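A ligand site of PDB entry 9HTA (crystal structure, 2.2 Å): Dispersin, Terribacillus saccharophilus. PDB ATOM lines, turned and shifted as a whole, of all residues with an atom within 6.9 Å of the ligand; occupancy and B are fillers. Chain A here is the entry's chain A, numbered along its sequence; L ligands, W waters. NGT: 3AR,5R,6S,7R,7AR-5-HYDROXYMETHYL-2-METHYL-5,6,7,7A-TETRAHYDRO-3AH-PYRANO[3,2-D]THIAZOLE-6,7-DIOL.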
ATOM      1  N   ASP A  10     -20.630  -7.412  17.933  1.00  0.00           N
ATOM      2  CA  ASP A  10     -19.884  -7.068  19.129  1.00  0.00           C
ATOM      3  C   ASP A  10     -20.694  -7.442  20.373  1.00  0.00           C
ATOM      4  O   ASP A  10     -21.475  -6.632  20.870  1.00  0.00           O
ATOM      5  CB  ASP A  10     -19.561  -5.583  19.078  1.00  0.00           C
ATOM      6  CG  ASP A  10     -18.717  -5.045  20.230  1.00  0.00           C
ATOM      7  OD1 ASP A  10     -18.340  -5.852  21.097  1.00  0.00           O
ATOM      8  OD2 ASP A  10     -18.470  -3.819  20.238  1.00  0.00           O
ATOM      9  N   ARG A  13     -18.753  -5.270  24.048  1.00  0.00           N
ATOM     10  CA  ARG A  13     -19.126  -3.956  24.542  1.00  0.00           C
ATOM     11  C   ARG A  13     -20.601  -3.892  24.958  1.00  0.00           C
ATOM     12  O   ARG A  13     -21.053  -2.888  25.519  1.00  0.00           O
ATOM     13  CB  ARG A  13     -18.857  -2.879  23.482  1.00  0.00           C
ATOM     14  CG  ARG A  13     -17.414  -2.415  23.319  1.00  0.00           C
ATOM     15  CD  ARG A  13     -16.426  -3.516  22.968  1.00  0.00           C
ATOM     16  NE  ARG A  13     -15.190  -2.881  22.508  1.00  0.00           N
ATOM     17  CZ  ARG A  13     -14.935  -2.454  21.266  1.00  0.00           C
ATOM     18  NH1 ARG A  13     -15.683  -2.883  20.263  1.00  0.00           N
ATOM     19  NH2 ARG A  13     -13.897  -1.670  21.028  1.00  0.00           N
ATOM     20  N   HIS A  39     -17.911 -11.372  17.825  1.00  0.00           N
ATOM     21  CA  HIS A  39     -16.847 -10.606  18.440  1.00  0.00           C
ATOM     22  C   HIS A  39     -17.078 -10.559  19.949  1.00  0.00           C
ATOM     23  O   HIS A  39     -17.678  -9.617  20.484  1.00  0.00           O
ATOM     24  CB  HIS A  39     -16.806  -9.228  17.781  1.00  0.00           C
ATOM     25  CG  HIS A  39     -15.704  -8.326  18.212  1.00  0.00           C
ATOM     26  ND1 HIS A  39     -14.511  -8.255  17.535  1.00  0.00           N
ATOM     27  CD2 HIS A  39     -15.640  -7.424  19.189  1.00  0.00           C
ATOM     28  CE1 HIS A  39     -13.745  -7.337  18.102  1.00  0.00           C
ATOM     29  NE2 HIS A  39     -14.418  -6.818  19.116  1.00  0.00           N
ATOM     30  N   ASP A  42     -12.928  -8.249  23.839  1.00  0.00           N
ATOM     31  CA  ASP A  42     -12.435  -6.905  23.628  1.00  0.00           C
ATOM     32  C   ASP A  42     -12.043  -6.327  24.983  1.00  0.00           C
ATOM     33  O   ASP A  42     -11.992  -7.045  25.984  1.00  0.00           O
ATOM     34  CB  ASP A  42     -13.442  -6.058  22.866  1.00  0.00           C
ATOM     35  CG  ASP A  42     -12.835  -4.979  21.980  1.00  0.00           C
ATOM     36  OD1 ASP A  42     -12.202  -4.055  22.543  1.00  0.00           O
ATOM     37  OD2 ASP A  42     -12.974  -5.089  20.746  1.00  0.00           O
ATOM     38  N   ASP A  89      -9.860 -10.960  19.811  1.00  0.00           N
ATOM     39  CA  ASP A  89      -9.020  -9.883  19.324  1.00  0.00           C
ATOM     40  C   ASP A  89      -7.645  -9.931  19.988  1.00  0.00           C
ATOM     41  O   ASP A  89      -7.511  -9.603  21.166  1.00  0.00           O
ATOM     42  CB  ASP A  89      -9.697  -8.540  19.531  1.00  0.00           C
ATOM     43  CG  ASP A  89      -9.229  -7.464  18.561  1.00  0.00           C
ATOM     44  OD1 ASP A  89      -7.992  -7.407  18.324  1.00  0.00           O
ATOM     45  OD2 ASP A  89     -10.092  -6.712  18.061  1.00  0.00           O
ATOM     46  N   HIS A  93      -6.958  -4.883  22.077  1.00  0.00           N
ATOM     47  CA  HIS A  93      -8.364  -5.110  22.393  1.00  0.00           C
ATOM     48  C   HIS A  93      -8.488  -6.360  23.285  1.00  0.00           C
ATOM     49  O   HIS A  93      -9.357  -7.209  23.058  1.00  0.00           O
ATOM     50  CB  HIS A  93      -9.219  -5.169  21.114  1.00  0.00           C
ATOM     51  CG  HIS A  93      -9.313  -3.854  20.409  1.00  0.00           C
ATOM     52  ND1 HIS A  93     -10.199  -2.879  20.803  1.00  0.00           N
ATOM     53  CD2 HIS A  93      -8.601  -3.337  19.402  1.00  0.00           C
ATOM     54  CE1 HIS A  93     -10.031  -1.810  20.020  1.00  0.00           C
ATOM     55  NE2 HIS A  93      -9.062  -2.073  19.158  1.00  0.00           N
ATOM     56  N   ASP A 160      -6.342  -5.500  14.927  1.00  0.00           N
ATOM     57  CA  ASP A 160      -6.761  -4.136  14.653  1.00  0.00           C
ATOM     58  C   ASP A 160      -6.203  -3.239  15.741  1.00  0.00           C
ATOM     59  O   ASP A 160      -6.168  -3.663  16.898  1.00  0.00           O
ATOM     60  CB  ASP A 160      -8.271  -4.035  14.545  1.00  0.00           C
ATOM     61  CG  ASP A 160      -9.042  -4.413  15.802  1.00  0.00           C
ATOM     62  OD1 ASP A 160      -8.833  -5.544  16.314  1.00  0.00           O
ATOM     63  OD2 ASP A 160      -9.811  -3.556  16.284  1.00  0.00           O
ATOM     64  N   GLU A 161      -5.739  -2.043  15.348  1.00  0.00           N
ATOM     65  CA  GLU A 161      -5.373  -0.915  16.198  1.00  0.00           C
ATOM     66  C   GLU A 161      -4.267  -1.300  17.188  1.00  0.00           C
ATOM     67  O   GLU A 161      -4.340  -0.954  18.370  1.00  0.00           O
ATOM     68  CB  GLU A 161      -6.576  -0.327  16.929  1.00  0.00           C
ATOM     69  CG  GLU A 161      -7.732   0.008  15.979  1.00  0.00           C
ATOM     70  CD  GLU A 161      -8.956   0.602  16.635  1.00  0.00           C
ATOM     71  OE1 GLU A 161      -9.337   0.190  17.763  1.00  0.00           O
ATOM     72  OE2 GLU A 161      -9.517   1.494  15.964  1.00  0.00           O
ATOM     73  N   TRP A 193      -8.009  -8.011  10.827  1.00  0.00           N
ATOM     74  CA  TRP A 193      -8.285  -6.718  10.225  1.00  0.00           C
ATOM     75  C   TRP A 193      -7.072  -6.243   9.406  1.00  0.00           C
ATOM     76  O   TRP A 193      -5.945  -6.745   9.596  1.00  0.00           O
ATOM     77  CB  TRP A 193      -8.673  -5.731  11.331  1.00  0.00           C
ATOM     78  CG  TRP A 193      -9.821  -6.244  12.147  1.00  0.00           C
ATOM     79  CD1 TRP A 193      -9.766  -6.920  13.335  1.00  0.00           C
ATOM     80  CD2 TRP A 193     -11.224  -6.136  11.832  1.00  0.00           C
ATOM     81  NE1 TRP A 193     -11.017  -7.232  13.774  1.00  0.00           N
ATOM     82  CE2 TRP A 193     -11.939  -6.767  12.872  1.00  0.00           C
ATOM     83  CE3 TRP A 193     -11.940  -5.558  10.767  1.00  0.00           C
ATOM     84  CZ2 TRP A 193     -13.331  -6.839  12.885  1.00  0.00           C
ATOM     85  CZ3 TRP A 193     -13.318  -5.628  10.777  1.00  0.00           C
ATOM     86  CH2 TRP A 193     -14.002  -6.278  11.816  1.00  0.00           C
ATOM     87  N   ASP A 195      -5.850  -3.033   9.181  1.00  0.00           N
ATOM     88  CA  ASP A 195      -5.355  -1.707   9.525  1.00  0.00           C
ATOM     89  C   ASP A 195      -3.912  -1.685  10.029  1.00  0.00           C
ATOM     90  O   ASP A 195      -3.277  -0.653   9.937  1.00  0.00           O
ATOM     91  CB  ASP A 195      -6.258  -1.031  10.545  1.00  0.00           C
ATOM     92  CG  ASP A 195      -6.524  -1.842  11.799  1.00  0.00           C
ATOM     93  OD1 ASP A 195      -6.958  -3.004  11.630  1.00  0.00           O
ATOM     94  OD2 ASP A 195      -6.273  -1.332  12.915  1.00  0.00           O
ATOM     95  N   LEU A 212      -9.934  -8.668   6.685  1.00  0.00           N
ATOM     96  CA  LEU A 212     -11.142  -7.923   6.931  1.00  0.00           C
ATOM     97  C   LEU A 212     -10.806  -6.464   6.688  1.00  0.00           C
ATOM     98  O   LEU A 212     -10.304  -5.777   7.585  1.00  0.00           O
ATOM     99  CB  LEU A 212     -11.646  -8.153   8.359  1.00  0.00           C
ATOM    100  CG  LEU A 212     -11.899  -9.605   8.785  1.00  0.00           C
ATOM    101  CD1 LEU A 212     -12.774  -9.614  10.026  1.00  0.00           C
ATOM    102  CD2 LEU A 212     -12.540 -10.479   7.705  1.00  0.00           C
ATOM    103  N   TRP A 214     -11.473  -2.797   6.412  1.00  0.00           N
ATOM    104  CA  TRP A 214     -12.499  -1.926   6.941  1.00  0.00           C
ATOM    105  C   TRP A 214     -12.156  -0.471   6.691  1.00  0.00           C
ATOM    106  O   TRP A 214     -13.058   0.349   6.523  1.00  0.00           O
ATOM    107  CB  TRP A 214     -12.776  -2.229   8.419  1.00  0.00           C
ATOM    108  CG  TRP A 214     -11.655  -1.920   9.358  1.00  0.00           C
ATOM    109  CD1 TRP A 214     -10.573  -2.703   9.588  1.00  0.00           C
ATOM    110  CD2 TRP A 214     -11.543  -0.794  10.252  1.00  0.00           C
ATOM    111  NE1 TRP A 214      -9.762  -2.121  10.518  1.00  0.00           N
ATOM    112  CE2 TRP A 214     -10.326  -0.947  10.952  1.00  0.00           C
ATOM    113  CE3 TRP A 214     -12.317   0.338  10.530  1.00  0.00           C
ATOM    114  CZ2 TRP A 214      -9.884  -0.029  11.900  1.00  0.00           C
ATOM    115  CZ3 TRP A 214     -11.892   1.235  11.490  1.00  0.00           C
ATOM    116  CH2 TRP A 214     -10.699   1.050  12.182  1.00  0.00           C
ATOM    117  N   ALA A 243     -16.101   0.745   6.851  1.00  0.00           N
ATOM    118  CA  ALA A 243     -16.380   1.402   8.114  1.00  0.00           C
ATOM    119  C   ALA A 243     -17.542   2.396   8.053  1.00  0.00           C
ATOM    120  O   ALA A 243     -18.064   2.757   9.103  1.00  0.00           O
ATOM    121  CB  ALA A 243     -15.148   2.104   8.633  1.00  0.00           C
ATOM    122  N   TYR A 247     -20.848  -0.347   8.937  1.00  0.00           N
ATOM    123  CA  TYR A 247     -20.727  -0.287  10.391  1.00  0.00           C
ATOM    124  C   TYR A 247     -21.976   0.399  10.916  1.00  0.00           C
ATOM    125  O   TYR A 247     -22.457   1.366  10.320  1.00  0.00           O
ATOM    126  CB  TYR A 247     -19.538   0.518  10.928  1.00  0.00           C
ATOM    127  CG  TYR A 247     -18.183  -0.187  11.008  1.00  0.00           C
ATOM    128  CD1 TYR A 247     -17.991  -1.477  10.543  1.00  0.00           C
ATOM    129  CD2 TYR A 247     -17.083   0.485  11.528  1.00  0.00           C
ATOM    130  CE1 TYR A 247     -16.756  -2.106  10.639  1.00  0.00           C
ATOM    131  CE2 TYR A 247     -15.828  -0.119  11.599  1.00  0.00           C
ATOM    132  CZ  TYR A 247     -15.668  -1.417  11.152  1.00  0.00           C
ATOM    133  OH  TYR A 247     -14.472  -2.073  11.206  1.00  0.00           O
ATOM    134  N   LEU A 249     -23.623   1.412  14.963  1.00  0.00           N
ATOM    135  CA  LEU A 249     -23.550   1.402  16.407  1.00  0.00           C
ATOM    136  C   LEU A 249     -24.952   1.621  16.967  1.00  0.00           C
ATOM    137  O   LEU A 249     -25.384   2.770  17.096  1.00  0.00           O
ATOM    138  CB  LEU A 249     -22.563   2.459  16.874  1.00  0.00           C
ATOM    139  CG  LEU A 249     -21.085   2.075  16.735  1.00  0.00           C
ATOM    140  CD1 LEU A 249     -20.670   2.011  15.262  1.00  0.00           C
ATOM    141  CD2 LEU A 249     -20.139   2.982  17.521  1.00  0.00           C
ATOM    142  N   TRP A 298     -21.264  -2.665  16.258  1.00  0.00           N
ATOM    143  CA  TRP A 298     -20.380  -2.383  17.386  1.00  0.00           C
ATOM    144  C   TRP A 298     -21.233  -1.963  18.599  1.00  0.00           C
ATOM    145  O   TRP A 298     -22.174  -1.204  18.442  1.00  0.00           O
ATOM    146  CB  TRP A 298     -19.325  -1.319  17.030  1.00  0.00           C
ATOM    147  CG  TRP A 298     -18.369  -1.775  15.950  1.00  0.00           C
ATOM    148  CD1 TRP A 298     -18.363  -1.406  14.648  1.00  0.00           C
ATOM    149  CD2 TRP A 298     -17.313  -2.742  16.104  1.00  0.00           C
ATOM    150  NE1 TRP A 298     -17.372  -2.063  13.967  1.00  0.00           N
ATOM    151  CE2 TRP A 298     -16.722  -2.896  14.828  1.00  0.00           C
ATOM    152  CE3 TRP A 298     -16.818  -3.502  17.182  1.00  0.00           C
ATOM    153  CZ2 TRP A 298     -15.655  -3.772  14.602  1.00  0.00           C
ATOM    154  CZ3 TRP A 298     -15.749  -4.348  16.957  1.00  0.00           C
ATOM    155  CH2 TRP A 298     -15.181  -4.484  15.693  1.00  0.00           C
ATOM    156  N   GLY A 299     -20.830  -2.413  19.789  1.00  0.00           N
ATOM    157  CA  GLY A 299     -21.642  -2.360  20.998  1.00  0.00           C
ATOM    158  C   GLY A 299     -21.481  -1.100  21.848  1.00  0.00           C
ATOM    159  O   GLY A 299     -22.331  -0.855  22.708  1.00  0.00           O
ATOM    160  N   GLU A 300     -20.467  -0.252  21.626  1.00  0.00           N
ATOM    161  CA  GLU A 300     -20.078   0.737  22.634  1.00  0.00           C
ATOM    162  C   GLU A 300     -21.049   1.925  22.759  1.00  0.00           C
ATOM    163  O   GLU A 300     -20.849   2.771  23.631  1.00  0.00           O
ATOM    164  CB  GLU A 300     -18.640   1.245  22.487  1.00  0.00           C
ATOM    165  CG  GLU A 300     -18.339   1.884  21.135  1.00  0.00           C
ATOM    166  CD  GLU A 300     -17.703   0.923  20.141  1.00  0.00           C
ATOM    167  OE1 GLU A 300     -18.280  -0.161  19.896  1.00  0.00           O
ATOM    168  OE2 GLU A 300     -16.610   1.263  19.655  1.00  0.00           O
ATOM    169  N   HIS A 301     -22.062   2.031  21.894  1.00  0.00           N
ATOM    170  CA  HIS A 301     -23.106   3.036  22.052  1.00  0.00           C
ATOM    171  C   HIS A 301     -24.403   2.416  22.547  1.00  0.00           C
ATOM    172  O   HIS A 301     -25.370   3.135  22.769  1.00  0.00           O
ATOM    173  CB  HIS A 301     -23.343   3.783  20.736  1.00  0.00           C
ATOM    174  CG  HIS A 301     -22.273   4.746  20.360  1.00  0.00           C
ATOM    175  ND1 HIS A 301     -22.240   5.366  19.127  1.00  0.00           N
ATOM    176  CD2 HIS A 301     -21.229   5.209  21.057  1.00  0.00           C
ATOM    177  CE1 HIS A 301     -21.208   6.192  19.096  1.00  0.00           C
ATOM    178  NE2 HIS A 301     -20.576   6.107  20.251  1.00  0.00           N
HETATM  179  C1  NGT L   1     -13.445   0.179  15.068  1.00  0.00           C
HETATM  180  C2  NGT L   1     -12.688  -0.636  16.129  1.00  0.00           C
HETATM  181  C3  NGT L   1     -13.732  -1.210  17.065  1.00  0.00           C
HETATM  182  C4  NGT L   1     -14.628  -0.104  17.609  1.00  0.00           C
HETATM  183  C5  NGT L   1     -15.282   0.781  16.538  1.00  0.00           C
HETATM  184  C6  NGT L   1     -14.988   2.260  16.682  1.00  0.00           C
HETATM  185  C7  NGT L   1     -12.231  -2.098  14.428  1.00  0.00           C
HETATM  186  C8  NGT L   1     -11.810  -3.309  13.654  1.00  0.00           C
HETATM  187  N2  NGT L   1     -11.868  -1.760  15.594  1.00  0.00           N
HETATM  188  S1  NGT L   1     -13.292  -0.976  13.713  1.00  0.00           S
HETATM  189  O3  NGT L   1     -13.038  -1.873  18.126  1.00  0.00           O
HETATM  190  O4  NGT L   1     -15.673  -0.746  18.344  1.00  0.00           O
HETATM  191  O5  NGT L   1     -14.823   0.389  15.230  1.00  0.00           O
HETATM  192  O6  NGT L   1     -16.027   2.960  17.380  1.00  0.00           O
HETATM  193  O   HOH W   1     -12.063  -4.315  18.139  1.00  0.00           O
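The side-chain carboxylate (OE2) of Glu 300 sits at hydrogen-bond distance from an oxygen (O4) of the ligand, 2.6 Å away. N2 of the ligand lies within hydrogen-bond range of OD2 of Asp 160. NH1 of Arg 13 is in hydrogen-bond range of O4 of the ligand (2.9 Å). The side-chain hydroxyl (OH) of Tyr 247 lies close to a sulfur (S1) of the ligand, 3.0 Å away.
OD2 of Asp 160 lies within hydrogen-bond range of NE2 of His 93 (3.3 Å). The side-chain carboxylate (OD1) of Asp 160 lies close to the side-chain carboxylate (OD2) of Asp 89, 2.4 Å away. NE of Arg 13 lies within salt-bridge range of OD1 of Asp 42, 3.2 Å away. The indole nitrogen (NE1) of Trp 214 sits at hydrogen-bond distance from the side-chain carboxylate (OD1) of Asp 195, at 3.1 Å. N of Ala 243 is in hydrogen-bond range of O of Trp 214 (3.1 Å). NE2 of His 93 sits at hydrogen-bond distance from OE1 of Glu 161 (2.7 Å). ND1 of His 93 sits at hydrogen-bond distance from OD1 of Asp 42, 2.9 Å away. N of Glu 161 sits at hydrogen-bond distance from OD2 of Asp 195 (2.6 Å).
CE1 of His 93 touches O3 of the ligand, 3.6 Å away. Glu 161 touches the ligand. Trp 193 touches the ligand. CZ3 of Trp 214 touches S1 of the ligand, at 3.4 Å. CE3 of Trp 298 touches O4 of the ligand, at 3.2 Å. Hydrophobic or aromatic side chains that line the ligand: His 93, Trp 193, Trp 214, Tyr 247 and Trp 298. Within 4 Å of the ligand: Arg 13, His 93, Asp 160, Glu 161, Trp 193, Trp 214, Tyr 247, Trp 298 and Glu 300.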
